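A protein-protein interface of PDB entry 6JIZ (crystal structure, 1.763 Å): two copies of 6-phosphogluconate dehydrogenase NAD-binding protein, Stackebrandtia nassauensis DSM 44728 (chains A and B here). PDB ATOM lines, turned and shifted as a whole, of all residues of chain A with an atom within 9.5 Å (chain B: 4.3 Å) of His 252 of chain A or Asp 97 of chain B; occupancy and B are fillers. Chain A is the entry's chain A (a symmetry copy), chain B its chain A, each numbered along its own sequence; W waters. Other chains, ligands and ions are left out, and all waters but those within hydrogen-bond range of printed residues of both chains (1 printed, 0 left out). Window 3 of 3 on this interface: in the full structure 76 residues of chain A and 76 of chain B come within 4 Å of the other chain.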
ATOM      1  N   HIS A 187     -24.583 -10.712  28.390  1.00  0.00           N
ATOM      2  CA  HIS A 187     -23.481 -11.158  29.241  1.00  0.00           C
ATOM      3  C   HIS A 187     -22.133 -10.825  28.606  1.00  0.00           C
ATOM      4  O   HIS A 187     -21.210 -10.330  29.278  1.00  0.00           O
ATOM      5  CB  HIS A 187     -23.597 -12.664  29.496  1.00  0.00           C
ATOM      6  CG  HIS A 187     -22.627 -13.154  30.525  1.00  0.00           C
ATOM      7  ND1 HIS A 187     -21.363 -13.600  30.201  1.00  0.00           N
ATOM      8  CD2 HIS A 187     -22.721 -13.225  31.874  1.00  0.00           C
ATOM      9  CE1 HIS A 187     -20.720 -13.931  31.307  1.00  0.00           C
ATOM     10  NE2 HIS A 187     -21.522 -13.715  32.337  1.00  0.00           N
ATOM     11  N   LEU A 191     -19.085  -8.499  29.969  1.00  0.00           N
ATOM     12  CA  LEU A 191     -17.714  -8.973  30.126  1.00  0.00           C
ATOM     13  C   LEU A 191     -16.722  -7.944  29.588  1.00  0.00           C
ATOM     14  O   LEU A 191     -15.718  -7.627  30.238  1.00  0.00           O
ATOM     15  CB  LEU A 191     -17.564 -10.317  29.402  1.00  0.00           C
ATOM     16  CG  LEU A 191     -16.359 -11.185  29.720  1.00  0.00           C
ATOM     17  CD1 LEU A 191     -16.491 -11.636  31.150  1.00  0.00           C
ATOM     18  CD2 LEU A 191     -16.311 -12.383  28.769  1.00  0.00           C
ATOM     19  N   VAL A 244     -13.564 -31.113  24.008  1.00  0.00           N
ATOM     20  CA  VAL A 244     -12.496 -30.722  24.921  1.00  0.00           C
ATOM     21  C   VAL A 244     -11.921 -29.362  24.527  1.00  0.00           C
ATOM     22  O   VAL A 244     -11.560 -28.559  25.395  1.00  0.00           O
ATOM     23  CB  VAL A 244     -11.420 -31.829  24.991  1.00  0.00           C
ATOM     24  CG1 VAL A 244     -10.626 -31.906  23.701  1.00  0.00           C
ATOM     25  CG2 VAL A 244     -10.524 -31.631  26.212  1.00  0.00           C
ATOM     26  N   MET A 245     -11.881 -29.050  23.231  1.00  0.00           N
ATOM     27  CA  MET A 245     -11.350 -27.759  22.801  1.00  0.00           C
ATOM     28  C   MET A 245     -12.311 -26.631  23.159  1.00  0.00           C
ATOM     29  O   MET A 245     -11.907 -25.596  23.706  1.00  0.00           O
ATOM     30  CB  MET A 245     -11.083 -27.787  21.296  1.00  0.00           C
ATOM     31  CG  MET A 245     -10.235 -26.638  20.775  1.00  0.00           C
ATOM     32  SD  MET A 245     -11.203 -25.196  20.270  1.00  0.00           S
ATOM     33  CE  MET A 245     -12.207 -25.901  18.969  1.00  0.00           C
ATOM     34  N   MET A 246     -13.594 -26.816  22.864  1.00  0.00           N
ATOM     35  CA  MET A 246     -14.559 -25.770  23.169  1.00  0.00           C
ATOM     36  C   MET A 246     -14.819 -25.664  24.668  1.00  0.00           C
ATOM     37  O   MET A 246     -15.102 -24.567  25.166  1.00  0.00           O
ATOM     38  CB  MET A 246     -15.829 -26.019  22.361  1.00  0.00           C
ATOM     39  CG  MET A 246     -15.650 -25.476  20.954  1.00  0.00           C
ATOM     40  SD  MET A 246     -16.717 -26.209  19.728  1.00  0.00           S
ATOM     41  CE  MET A 246     -18.239 -25.297  20.045  1.00  0.00           C
ATOM     42  N   GLY A 247     -14.678 -26.770  25.402  1.00  0.00           N
ATOM     43  CA  GLY A 247     -14.778 -26.709  26.854  1.00  0.00           C
ATOM     44  C   GLY A 247     -13.658 -25.902  27.486  1.00  0.00           C
ATOM     45  O   GLY A 247     -13.859 -25.228  28.503  1.00  0.00           O
ATOM     46  N   ALA A 248     -12.457 -25.969  26.902  1.00  0.00           N
ATOM     47  CA  ALA A 248     -11.361 -25.134  27.394  1.00  0.00           C
ATOM     48  C   ALA A 248     -11.706 -23.661  27.253  1.00  0.00           C
ATOM     49  O   ALA A 248     -11.415 -22.853  28.145  1.00  0.00           O
ATOM     50  CB  ALA A 248     -10.067 -25.444  26.636  1.00  0.00           C
ATOM     51  N   THR A 249     -12.327 -23.296  26.130  1.00  0.00           N
ATOM     52  CA  THR A 249     -12.774 -21.922  25.935  1.00  0.00           C
ATOM     53  C   THR A 249     -13.874 -21.563  26.925  1.00  0.00           C
ATOM     54  O   THR A 249     -13.886 -20.455  27.470  1.00  0.00           O
ATOM     55  CB  THR A 249     -13.252 -21.736  24.495  1.00  0.00           C
ATOM     56  OG1 THR A 249     -12.124 -21.819  23.613  1.00  0.00           O
ATOM     57  CG2 THR A 249     -13.939 -20.375  24.300  1.00  0.00           C
ATOM     58  N   ALA A 250     -14.814 -22.481  27.166  1.00  0.00           N
ATOM     59  CA  ALA A 250     -15.821 -22.234  28.196  1.00  0.00           C
ATOM     60  C   ALA A 250     -15.176 -21.965  29.551  1.00  0.00           C
ATOM     61  O   ALA A 250     -15.638 -21.098  30.305  1.00  0.00           O
ATOM     62  CB  ALA A 250     -16.789 -23.421  28.289  1.00  0.00           C
ATOM     63  N   ASP A 251     -14.102 -22.698  29.882  1.00  0.00           N
ATOM     64  CA  ASP A 251     -13.394 -22.456  31.137  1.00  0.00           C
ATOM     65  C   ASP A 251     -12.774 -21.063  31.177  1.00  0.00           C
ATOM     66  O   ASP A 251     -12.782 -20.409  32.228  1.00  0.00           O
ATOM     67  CB  ASP A 251     -12.303 -23.508  31.341  1.00  0.00           C
ATOM     68  CG  ASP A 251     -12.861 -24.882  31.626  1.00  0.00           C
ATOM     69  OD1 ASP A 251     -14.082 -24.997  31.864  1.00  0.00           O
ATOM     70  OD2 ASP A 251     -12.068 -25.851  31.618  1.00  0.00           O
ATOM     71  N   HIS A 252     -12.208 -20.608  30.054  1.00  0.00           N
ATOM     72  CA  HIS A 252     -11.596 -19.276  30.003  1.00  0.00           C
ATOM     73  C   HIS A 252     -12.649 -18.183  30.139  1.00  0.00           C
ATOM     74  O   HIS A 252     -12.388 -17.126  30.724  1.00  0.00           O
ATOM     75  CB  HIS A 252     -10.820 -19.097  28.693  1.00  0.00           C
ATOM     76  CG  HIS A 252      -9.635 -20.010  28.545  1.00  0.00           C
ATOM     77  ND1 HIS A 252      -8.842 -20.386  29.609  1.00  0.00           N
ATOM     78  CD2 HIS A 252      -9.104 -20.601  27.449  1.00  0.00           C
ATOM     79  CE1 HIS A 252      -7.877 -21.180  29.175  1.00  0.00           C
ATOM     80  NE2 HIS A 252      -8.010 -21.323  27.868  1.00  0.00           N
ATOM     81  N   ILE A 253     -13.848 -18.410  29.597  1.00  0.00           N
ATOM     82  CA  ILE A 253     -14.911 -17.426  29.776  1.00  0.00           C
ATOM     83  C   ILE A 253     -15.302 -17.316  31.248  1.00  0.00           C
ATOM     84  O   ILE A 253     -15.506 -16.211  31.764  1.00  0.00           O
ATOM     85  CB  ILE A 253     -16.121 -17.780  28.891  1.00  0.00           C
ATOM     86  CG1 ILE A 253     -15.721 -17.714  27.416  1.00  0.00           C
ATOM     87  CG2 ILE A 253     -17.316 -16.835  29.196  1.00  0.00           C
ATOM     88  CD1 ILE A 253     -16.697 -18.427  26.478  1.00  0.00           C
ATOM     89  N   VAL A 254     -15.394 -18.451  31.950  1.00  0.00           N
ATOM     90  CA  VAL A 254     -15.711 -18.421  33.378  1.00  0.00           C
ATOM     91  C   VAL A 254     -14.619 -17.696  34.165  1.00  0.00           C
ATOM     92  O   VAL A 254     -14.913 -16.875  35.045  1.00  0.00           O
ATOM     93  CB  VAL A 254     -15.945 -19.846  33.908  1.00  0.00           C
ATOM     94  CG1 VAL A 254     -15.990 -19.846  35.438  1.00  0.00           C
ATOM     95  CG2 VAL A 254     -17.245 -20.421  33.329  1.00  0.00           C
ATOM     96  N   SER A 255     -13.345 -17.969  33.866  1.00  0.00           N
ATOM     97  CA  SER A 255     -12.306 -17.268  34.622  1.00  0.00           C
ATOM     98  C   SER A 255     -12.284 -15.778  34.292  1.00  0.00           C
ATOM     99  O   SER A 255     -12.029 -14.953  35.179  1.00  0.00           O
ATOM    100  CB  SER A 255     -10.927 -17.894  34.378  1.00  0.00           C
ATOM    101  OG  SER A 255     -10.550 -17.795  33.027  1.00  0.00           O
ATOM    102  N   ALA A 256     -12.552 -15.410  33.036  1.00  0.00           N
ATOM    103  CA  ALA A 256     -12.605 -13.993  32.687  1.00  0.00           C
ATOM    104  C   ALA A 256     -13.738 -13.298  33.432  1.00  0.00           C
ATOM    105  O   ALA A 256     -13.558 -12.200  33.973  1.00  0.00           O
ATOM    106  CB  ALA A 256     -12.763 -13.819  31.179  1.00  0.00           C
ATOM    107  N   ALA A 257     -14.909 -13.938  33.492  1.00  0.00           N
ATOM    108  CA  ALA A 257     -16.038 -13.340  34.205  1.00  0.00           C
ATOM    109  C   ALA A 257     -15.755 -13.253  35.696  1.00  0.00           C
ATOM    110  O   ALA A 257     -16.041 -12.231  36.333  1.00  0.00           O
ATOM    111  CB  ALA A 257     -17.314 -14.145  33.945  1.00  0.00           C
ATOM    112  N   LYS A 258     -15.180 -14.310  36.261  1.00  0.00           N
ATOM    113  CA  LYS A 258     -14.854 -14.311  37.680  1.00  0.00           C
ATOM    114  C   LYS A 258     -13.871 -13.198  38.010  1.00  0.00           C
ATOM    115  O   LYS A 258     -13.999 -12.532  39.044  1.00  0.00           O
ATOM    116  CB  LYS A 258     -14.288 -15.675  38.069  1.00  0.00           C
ATOM    117  CG  LYS A 258     -14.282 -15.979  39.552  1.00  0.00           C
ATOM    118  CD  LYS A 258     -13.871 -17.427  39.781  1.00  0.00           C
ATOM    119  CE  LYS A 258     -14.776 -18.380  38.997  1.00  0.00           C
ATOM    120  NZ  LYS A 258     -14.312 -19.798  39.059  1.00  0.00           N
ATOM    121  N   GLY A 259     -12.899 -12.967  37.129  1.00  0.00           N
ATOM    122  CA  GLY A 259     -11.882 -11.967  37.405  1.00  0.00           C
ATOM    123  C   GLY A 259     -12.397 -10.545  37.345  1.00  0.00           C
ATOM    124  O   GLY A 259     -11.865  -9.662  38.025  1.00  0.00           O
ATOM    125  N   SER A 260     -13.440 -10.299  36.551  1.00  0.00           N
ATOM    126  CA  SER A 260     -13.948  -8.949  36.344  1.00  0.00           C
ATOM    127  C   SER A 260     -15.240  -8.667  37.100  1.00  0.00           C
ATOM    128  O   SER A 260     -15.803  -7.580  36.949  1.00  0.00           O
ATOM    129  CB  SER A 260     -14.148  -8.684  34.853  1.00  0.00           C
ATOM    130  OG  SER A 260     -15.002  -9.647  34.279  1.00  0.00           O
ATOM    131  N   LEU A 264     -21.877 -15.030  37.061  1.00  0.00           N
ATOM    132  CA  LEU A 264     -21.322 -16.300  36.606  1.00  0.00           C
ATOM    133  C   LEU A 264     -22.348 -17.343  36.181  1.00  0.00           C
ATOM    134  O   LEU A 264     -21.952 -18.344  35.575  1.00  0.00           O
ATOM    135  CB  LEU A 264     -20.436 -16.908  37.701  1.00  0.00           C
ATOM    136  CG  LEU A 264     -19.151 -16.125  37.979  1.00  0.00           C
ATOM    137  CD1 LEU A 264     -18.455 -16.655  39.220  1.00  0.00           C
ATOM    138  CD2 LEU A 264     -18.240 -16.222  36.772  1.00  0.00           C
ATOM    139  N   PRO A 267     -22.282 -18.421  32.148  1.00  0.00           N
ATOM    140  CA  PRO A 267     -21.098 -19.163  31.667  1.00  0.00           C
ATOM    141  C   PRO A 267     -20.813 -20.420  32.473  1.00  0.00           C
ATOM    142  O   PRO A 267     -20.248 -21.380  31.929  1.00  0.00           O
ATOM    143  CB  PRO A 267     -19.957 -18.134  31.777  1.00  0.00           C
ATOM    144  CG  PRO A 267     -20.420 -17.151  32.824  1.00  0.00           C
ATOM    145  CD  PRO A 267     -21.926 -17.057  32.591  1.00  0.00           C
ATOM    146  N   VAL A 270     -22.803 -23.224  30.839  1.00  0.00           N
ATOM    147  CA  VAL A 270     -22.145 -23.720  29.634  1.00  0.00           C
ATOM    148  C   VAL A 270     -20.953 -24.589  30.011  1.00  0.00           C
ATOM    149  O   VAL A 270     -20.762 -25.685  29.465  1.00  0.00           O
ATOM    150  CB  VAL A 270     -21.728 -22.542  28.729  1.00  0.00           C
ATOM    151  CG1 VAL A 270     -20.847 -23.026  27.571  1.00  0.00           C
ATOM    152  CG2 VAL A 270     -22.971 -21.783  28.189  1.00  0.00           C
ATOM    153  N   LYS A 271     -20.140 -24.120  30.962  1.00  0.00           N
ATOM    154  CA  LYS A 271     -19.000 -24.916  31.417  1.00  0.00           C
ATOM    155  C   LYS A 271     -19.451 -26.254  31.992  1.00  0.00           C
ATOM    156  O   LYS A 271     -18.815 -27.287  31.749  1.00  0.00           O
ATOM    157  CB  LYS A 271     -18.188 -24.114  32.439  1.00  0.00           C
ATOM    158  CG  LYS A 271     -17.099 -24.902  33.174  1.00  0.00           C
ATOM    159  CD  LYS A 271     -16.292 -23.991  34.107  1.00  0.00           C
ATOM    160  CE  LYS A 271     -15.527 -24.786  35.181  1.00  0.00           C
ATOM    161  NZ  LYS A 271     -14.773 -25.933  34.595  1.00  0.00           N
ATOM    162  N   ASP A 275     -18.020 -29.705  30.801  1.00  0.00           N
ATOM    163  CA  ASP A 275     -17.342 -30.528  31.802  1.00  0.00           C
ATOM    164  C   ASP A 275     -17.916 -31.938  31.814  1.00  0.00           C
ATOM    165  O   ASP A 275     -17.174 -32.929  31.795  1.00  0.00           O
ATOM    166  CB  ASP A 275     -17.469 -29.900  33.192  1.00  0.00           C
ATOM    167  CG  ASP A 275     -16.483 -28.756  33.428  1.00  0.00           C
ATOM    168  OD1 ASP A 275     -15.668 -28.463  32.533  1.00  0.00           O
ATOM    169  OD2 ASP A 275     -16.524 -28.149  34.521  1.00  0.00           O
ATOM    170  N   ASP B  71      -2.623 -22.906  24.357  1.00  0.00           N
ATOM    171  CA  ASP B  71      -2.824 -21.957  25.451  1.00  0.00           C
ATOM    172  C   ASP B  71      -1.486 -21.303  25.779  1.00  0.00           C
ATOM    173  O   ASP B  71      -0.460 -21.616  25.172  1.00  0.00           O
ATOM    174  CB  ASP B  71      -3.444 -22.638  26.676  1.00  0.00           C
ATOM    175  CG  ASP B  71      -2.629 -23.826  27.176  1.00  0.00           C
ATOM    176  OD1 ASP B  71      -1.398 -23.871  26.975  1.00  0.00           O
ATOM    177  OD2 ASP B  71      -3.232 -24.741  27.776  1.00  0.00           O
ATOM    178  N   TYR B  72      -1.500 -20.377  26.742  1.00  0.00           N
ATOM    179  CA  TYR B  72      -0.259 -19.666  27.039  1.00  0.00           C
ATOM    180  C   TYR B  72       0.742 -20.539  27.790  1.00  0.00           C
ATOM    181  O   TYR B  72       1.952 -20.298  27.702  1.00  0.00           O
ATOM    182  CB  TYR B  72      -0.550 -18.384  27.827  1.00  0.00           C
ATOM    183  CG  TYR B  72      -0.822 -17.173  26.950  1.00  0.00           C
ATOM    184  CD1 TYR B  72      -1.691 -17.249  25.860  1.00  0.00           C
ATOM    185  CD2 TYR B  72      -0.215 -15.943  27.206  1.00  0.00           C
ATOM    186  CE1 TYR B  72      -1.938 -16.151  25.062  1.00  0.00           C
ATOM    187  CE2 TYR B  72      -0.469 -14.835  26.408  1.00  0.00           C
ATOM    188  CZ  TYR B  72      -1.337 -14.945  25.345  1.00  0.00           C
ATOM    189  OH  TYR B  72      -1.593 -13.864  24.533  1.00  0.00           O
ATOM    190  N   SER B  95      -2.821 -17.299  20.590  1.00  0.00           N
ATOM    191  CA  SER B  95      -3.439 -18.398  21.318  1.00  0.00           C
ATOM    192  C   SER B  95      -4.517 -17.883  22.263  1.00  0.00           C
ATOM    193  O   SER B  95      -4.396 -16.797  22.826  1.00  0.00           O
ATOM    194  CB  SER B  95      -2.392 -19.149  22.143  1.00  0.00           C
ATOM    195  OG  SER B  95      -1.203 -19.341  21.381  1.00  0.00           O
ATOM    196  N   SER B  96      -5.561 -18.686  22.460  1.00  0.00           N
ATOM    197  CA  SER B  96      -6.632 -18.281  23.355  1.00  0.00           C
ATOM    198  C   SER B  96      -6.288 -18.603  24.803  1.00  0.00           C
ATOM    199  O   SER B  96      -5.720 -19.657  25.113  1.00  0.00           O
ATOM    200  CB  SER B  96      -7.951 -18.952  22.978  1.00  0.00           C
ATOM    201  OG  SER B  96      -8.993 -18.384  23.755  1.00  0.00           O
ATOM    202  N   ASP B  97      -6.621 -17.675  25.691  1.00  0.00           N
ATOM    203  CA  ASP B  97      -6.420 -17.885  27.118  1.00  0.00           C
ATOM    204  C   ASP B  97      -7.148 -16.785  27.882  1.00  0.00           C
ATOM    205  O   ASP B  97      -7.694 -15.849  27.296  1.00  0.00           O
ATOM    206  CB  ASP B  97      -4.925 -17.909  27.479  1.00  0.00           C
ATOM    207  CG  ASP B  97      -4.615 -18.893  28.588  1.00  0.00           C
ATOM    208  OD1 ASP B  97      -5.356 -18.913  29.592  1.00  0.00           O
ATOM    209  OD2 ASP B  97      -3.634 -19.661  28.456  1.00  0.00           O
ATOM    210  N   ASP B  98      -7.132 -16.920  29.207  1.00  0.00           N
ATOM    211  CA  ASP B  98      -7.735 -15.949  30.112  1.00  0.00           C
ATOM    212  C   ASP B  98      -7.065 -14.581  29.949  1.00  0.00           C
ATOM    213  O   ASP B  98      -5.841 -14.510  29.786  1.00  0.00           O
ATOM    214  CB  ASP B  98      -7.578 -16.472  31.544  1.00  0.00           C
ATOM    215  CG  ASP B  98      -7.918 -15.446  32.598  1.00  0.00           C
ATOM    216  OD1 ASP B  98      -9.103 -15.364  32.997  1.00  0.00           O
ATOM    217  OD2 ASP B  98      -6.989 -14.738  33.044  1.00  0.00           O
ATOM    218  N   PRO B  99      -7.827 -13.475  29.974  1.00  0.00           N
ATOM    219  CA  PRO B  99      -7.194 -12.161  29.728  1.00  0.00           C
ATOM    220  C   PRO B  99      -6.099 -11.807  30.724  1.00  0.00           C
ATOM    221  O   PRO B  99      -5.059 -11.255  30.337  1.00  0.00           O
ATOM    222  CB  PRO B  99      -8.372 -11.180  29.818  1.00  0.00           C
ATOM    223  CG  PRO B  99      -9.577 -12.022  29.367  1.00  0.00           C
ATOM    224  CD  PRO B  99      -9.306 -13.394  29.969  1.00  0.00           C
ATOM    225  N   VAL B 101      -4.196 -13.901  32.297  1.00  0.00           N
ATOM    226  CA  VAL B 101      -3.039 -14.715  31.917  1.00  0.00           C
ATOM    227  C   VAL B 101      -2.237 -14.026  30.823  1.00  0.00           C
ATOM    228  O   VAL B 101      -1.002 -13.989  30.878  1.00  0.00           O
ATOM    229  CB  VAL B 101      -3.482 -16.131  31.489  1.00  0.00           C
ATOM    230  CG1 VAL B 101      -2.312 -16.873  30.811  1.00  0.00           C
ATOM    231  CG2 VAL B 101      -3.978 -16.903  32.691  1.00  0.00           C
ATOM    232  N   GLN B 168      -7.910 -11.005  23.985  1.00  0.00           N
ATOM    233  CA  GLN B 168      -8.589 -12.208  24.453  1.00  0.00           C
ATOM    234  C   GLN B 168      -9.887 -11.882  25.185  1.00  0.00           C
ATOM    235  O   GLN B 168     -10.801 -12.713  25.194  1.00  0.00           O
ATOM    236  CB  GLN B 168      -7.648 -13.055  25.324  1.00  0.00           C
ATOM    237  CG  GLN B 168      -6.614 -13.802  24.442  1.00  0.00           C
ATOM    238  CD  GLN B 168      -7.306 -14.722  23.439  1.00  0.00           C
ATOM    239  OE1 GLN B 168      -8.160 -15.509  23.825  1.00  0.00           O
ATOM    240  NE2 GLN B 168      -6.975 -14.594  22.157  1.00  0.00           N
ATOM    241  N   LEU B 172     -12.998 -13.879  23.886  1.00  0.00           N
ATOM    242  CA  LEU B 172     -13.810 -14.725  24.759  1.00  0.00           C
ATOM    243  C   LEU B 172     -15.238 -14.217  24.873  1.00  0.00           C
ATOM    244  O   LEU B 172     -16.161 -15.013  25.060  1.00  0.00           O
ATOM    245  CB  LEU B 172     -13.187 -14.818  26.147  1.00  0.00           C
ATOM    246  CG  LEU B 172     -11.801 -15.466  26.181  1.00  0.00           C
ATOM    247  CD1 LEU B 172     -11.254 -15.319  27.586  1.00  0.00           C
ATOM    248  CD2 LEU B 172     -11.909 -16.941  25.784  1.00  0.00           C
HETATM  249  O   HOH W   1      -7.273 -22.115  25.229  1.00  0.00           O
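Met 246 of chain A touches none of the printed residues of chain B. Printed residues of chain B within 4 Å of His 252 of chain A: Ser 96 (3.95 Å), Asp 97 (3.4 Å), Asp 98 (3.9 Å) and Leu 172 (3.8 Å). Val 254 of chain A touches none of the printed residues of chain B. Of the printed residues of chain B, Ser 255 of chain A touches Asp 98. No residue of chain A comes within 4 Å of Asp 71 of chain B. Of chain A, only His 252 (3.4 Å) comes within 4 Å of Asp 97 of chain B. Printed residues of chain A within 4 Å of Asp 98 of chain B: His 252, Ser 255 and Ala 256. Of the printed residues of chain A, Leu 172 of chain B touches His 252 and Ile 253. The nearest residue of chain A that does not touch Asp 97 of chain B is Ser 255 of chain A (6.3 Å). The nearest printed residue of chain A that does not touch Leu 172 of chain B is Ala 256 of chain A (4.2 Å).
Water W1 lies within hydrogen-bond range of NE2 of His 252 of chain A and O of Ser 96 of chain B.
OD2 of Asp 98 of chain B is in hydrogen-bond range of N of Val 101 of chain B (3.0 Å). OG of Ser 260 of chain A lies within hydrogen-bond range of O of Ala 256 of chain A (2.9 Å). The backbone NH (N) of Tyr 72 of chain B sits at hydrogen-bond distance from the side-chain carboxylate (OD2) of Asp 97 of chain B (2.8 Å). The side-chain hydroxyl (OG) of Ser 255 of chain A lies within hydrogen-bond range of the backbone carbonyl oxygen (O) of His 252 of chain A (3.0 Å). The side-chain hydroxyl (OG) of Ser 96 of chain B lies within hydrogen-bond range of the side-chain amide oxygen (OE1) of Gln 168 of chain B (3.0 Å). N of Asp 97 of chain B is in hydrogen-bond range of OE1 of Gln 168 of chain B, 3.2 Å away.
Hydrophobic or aromatic side chains of chain A within 4 Å of the printed part of chain B: His 252, Ile 253 and Ala 256. Hydrophobic or aromatic side chains of chain B within 4 Å of the printed part of chain A: Pro 99 and Leu 172. Among the printed residues, no Asp or Glu carboxylate lies within 4 Å of a Lys or Arg side-chain nitrogen of the other chain.
His 252 of chain A touches Ser 96 of chain B. CE1 of His 252 of chain A touches OD1 of Asp 97 of chain B (3.4 Å). ND1 of His 252 of chain A touches N of Asp 98 of chain B, 3.9 Å away. Leu 172 of chain B touches His 252 of chain A (CD2 to CB, 3.8 Å). Leu 172 of chain B touches Ile 253 of chain A. Ala 256 of chain A touches Pro 99 of chain B.
No position is printed for both chains.
OD1 of Asp 98 of chain B lies within hydrogen-bond range of OG of Ser 255 of chain A (2.8 Å). The backbone NH (N) of Ala 256 of chain A lies within hydrogen-bond range of the side-chain carboxylate (OD1) of Asp 98 of chain B (3.4 Å).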
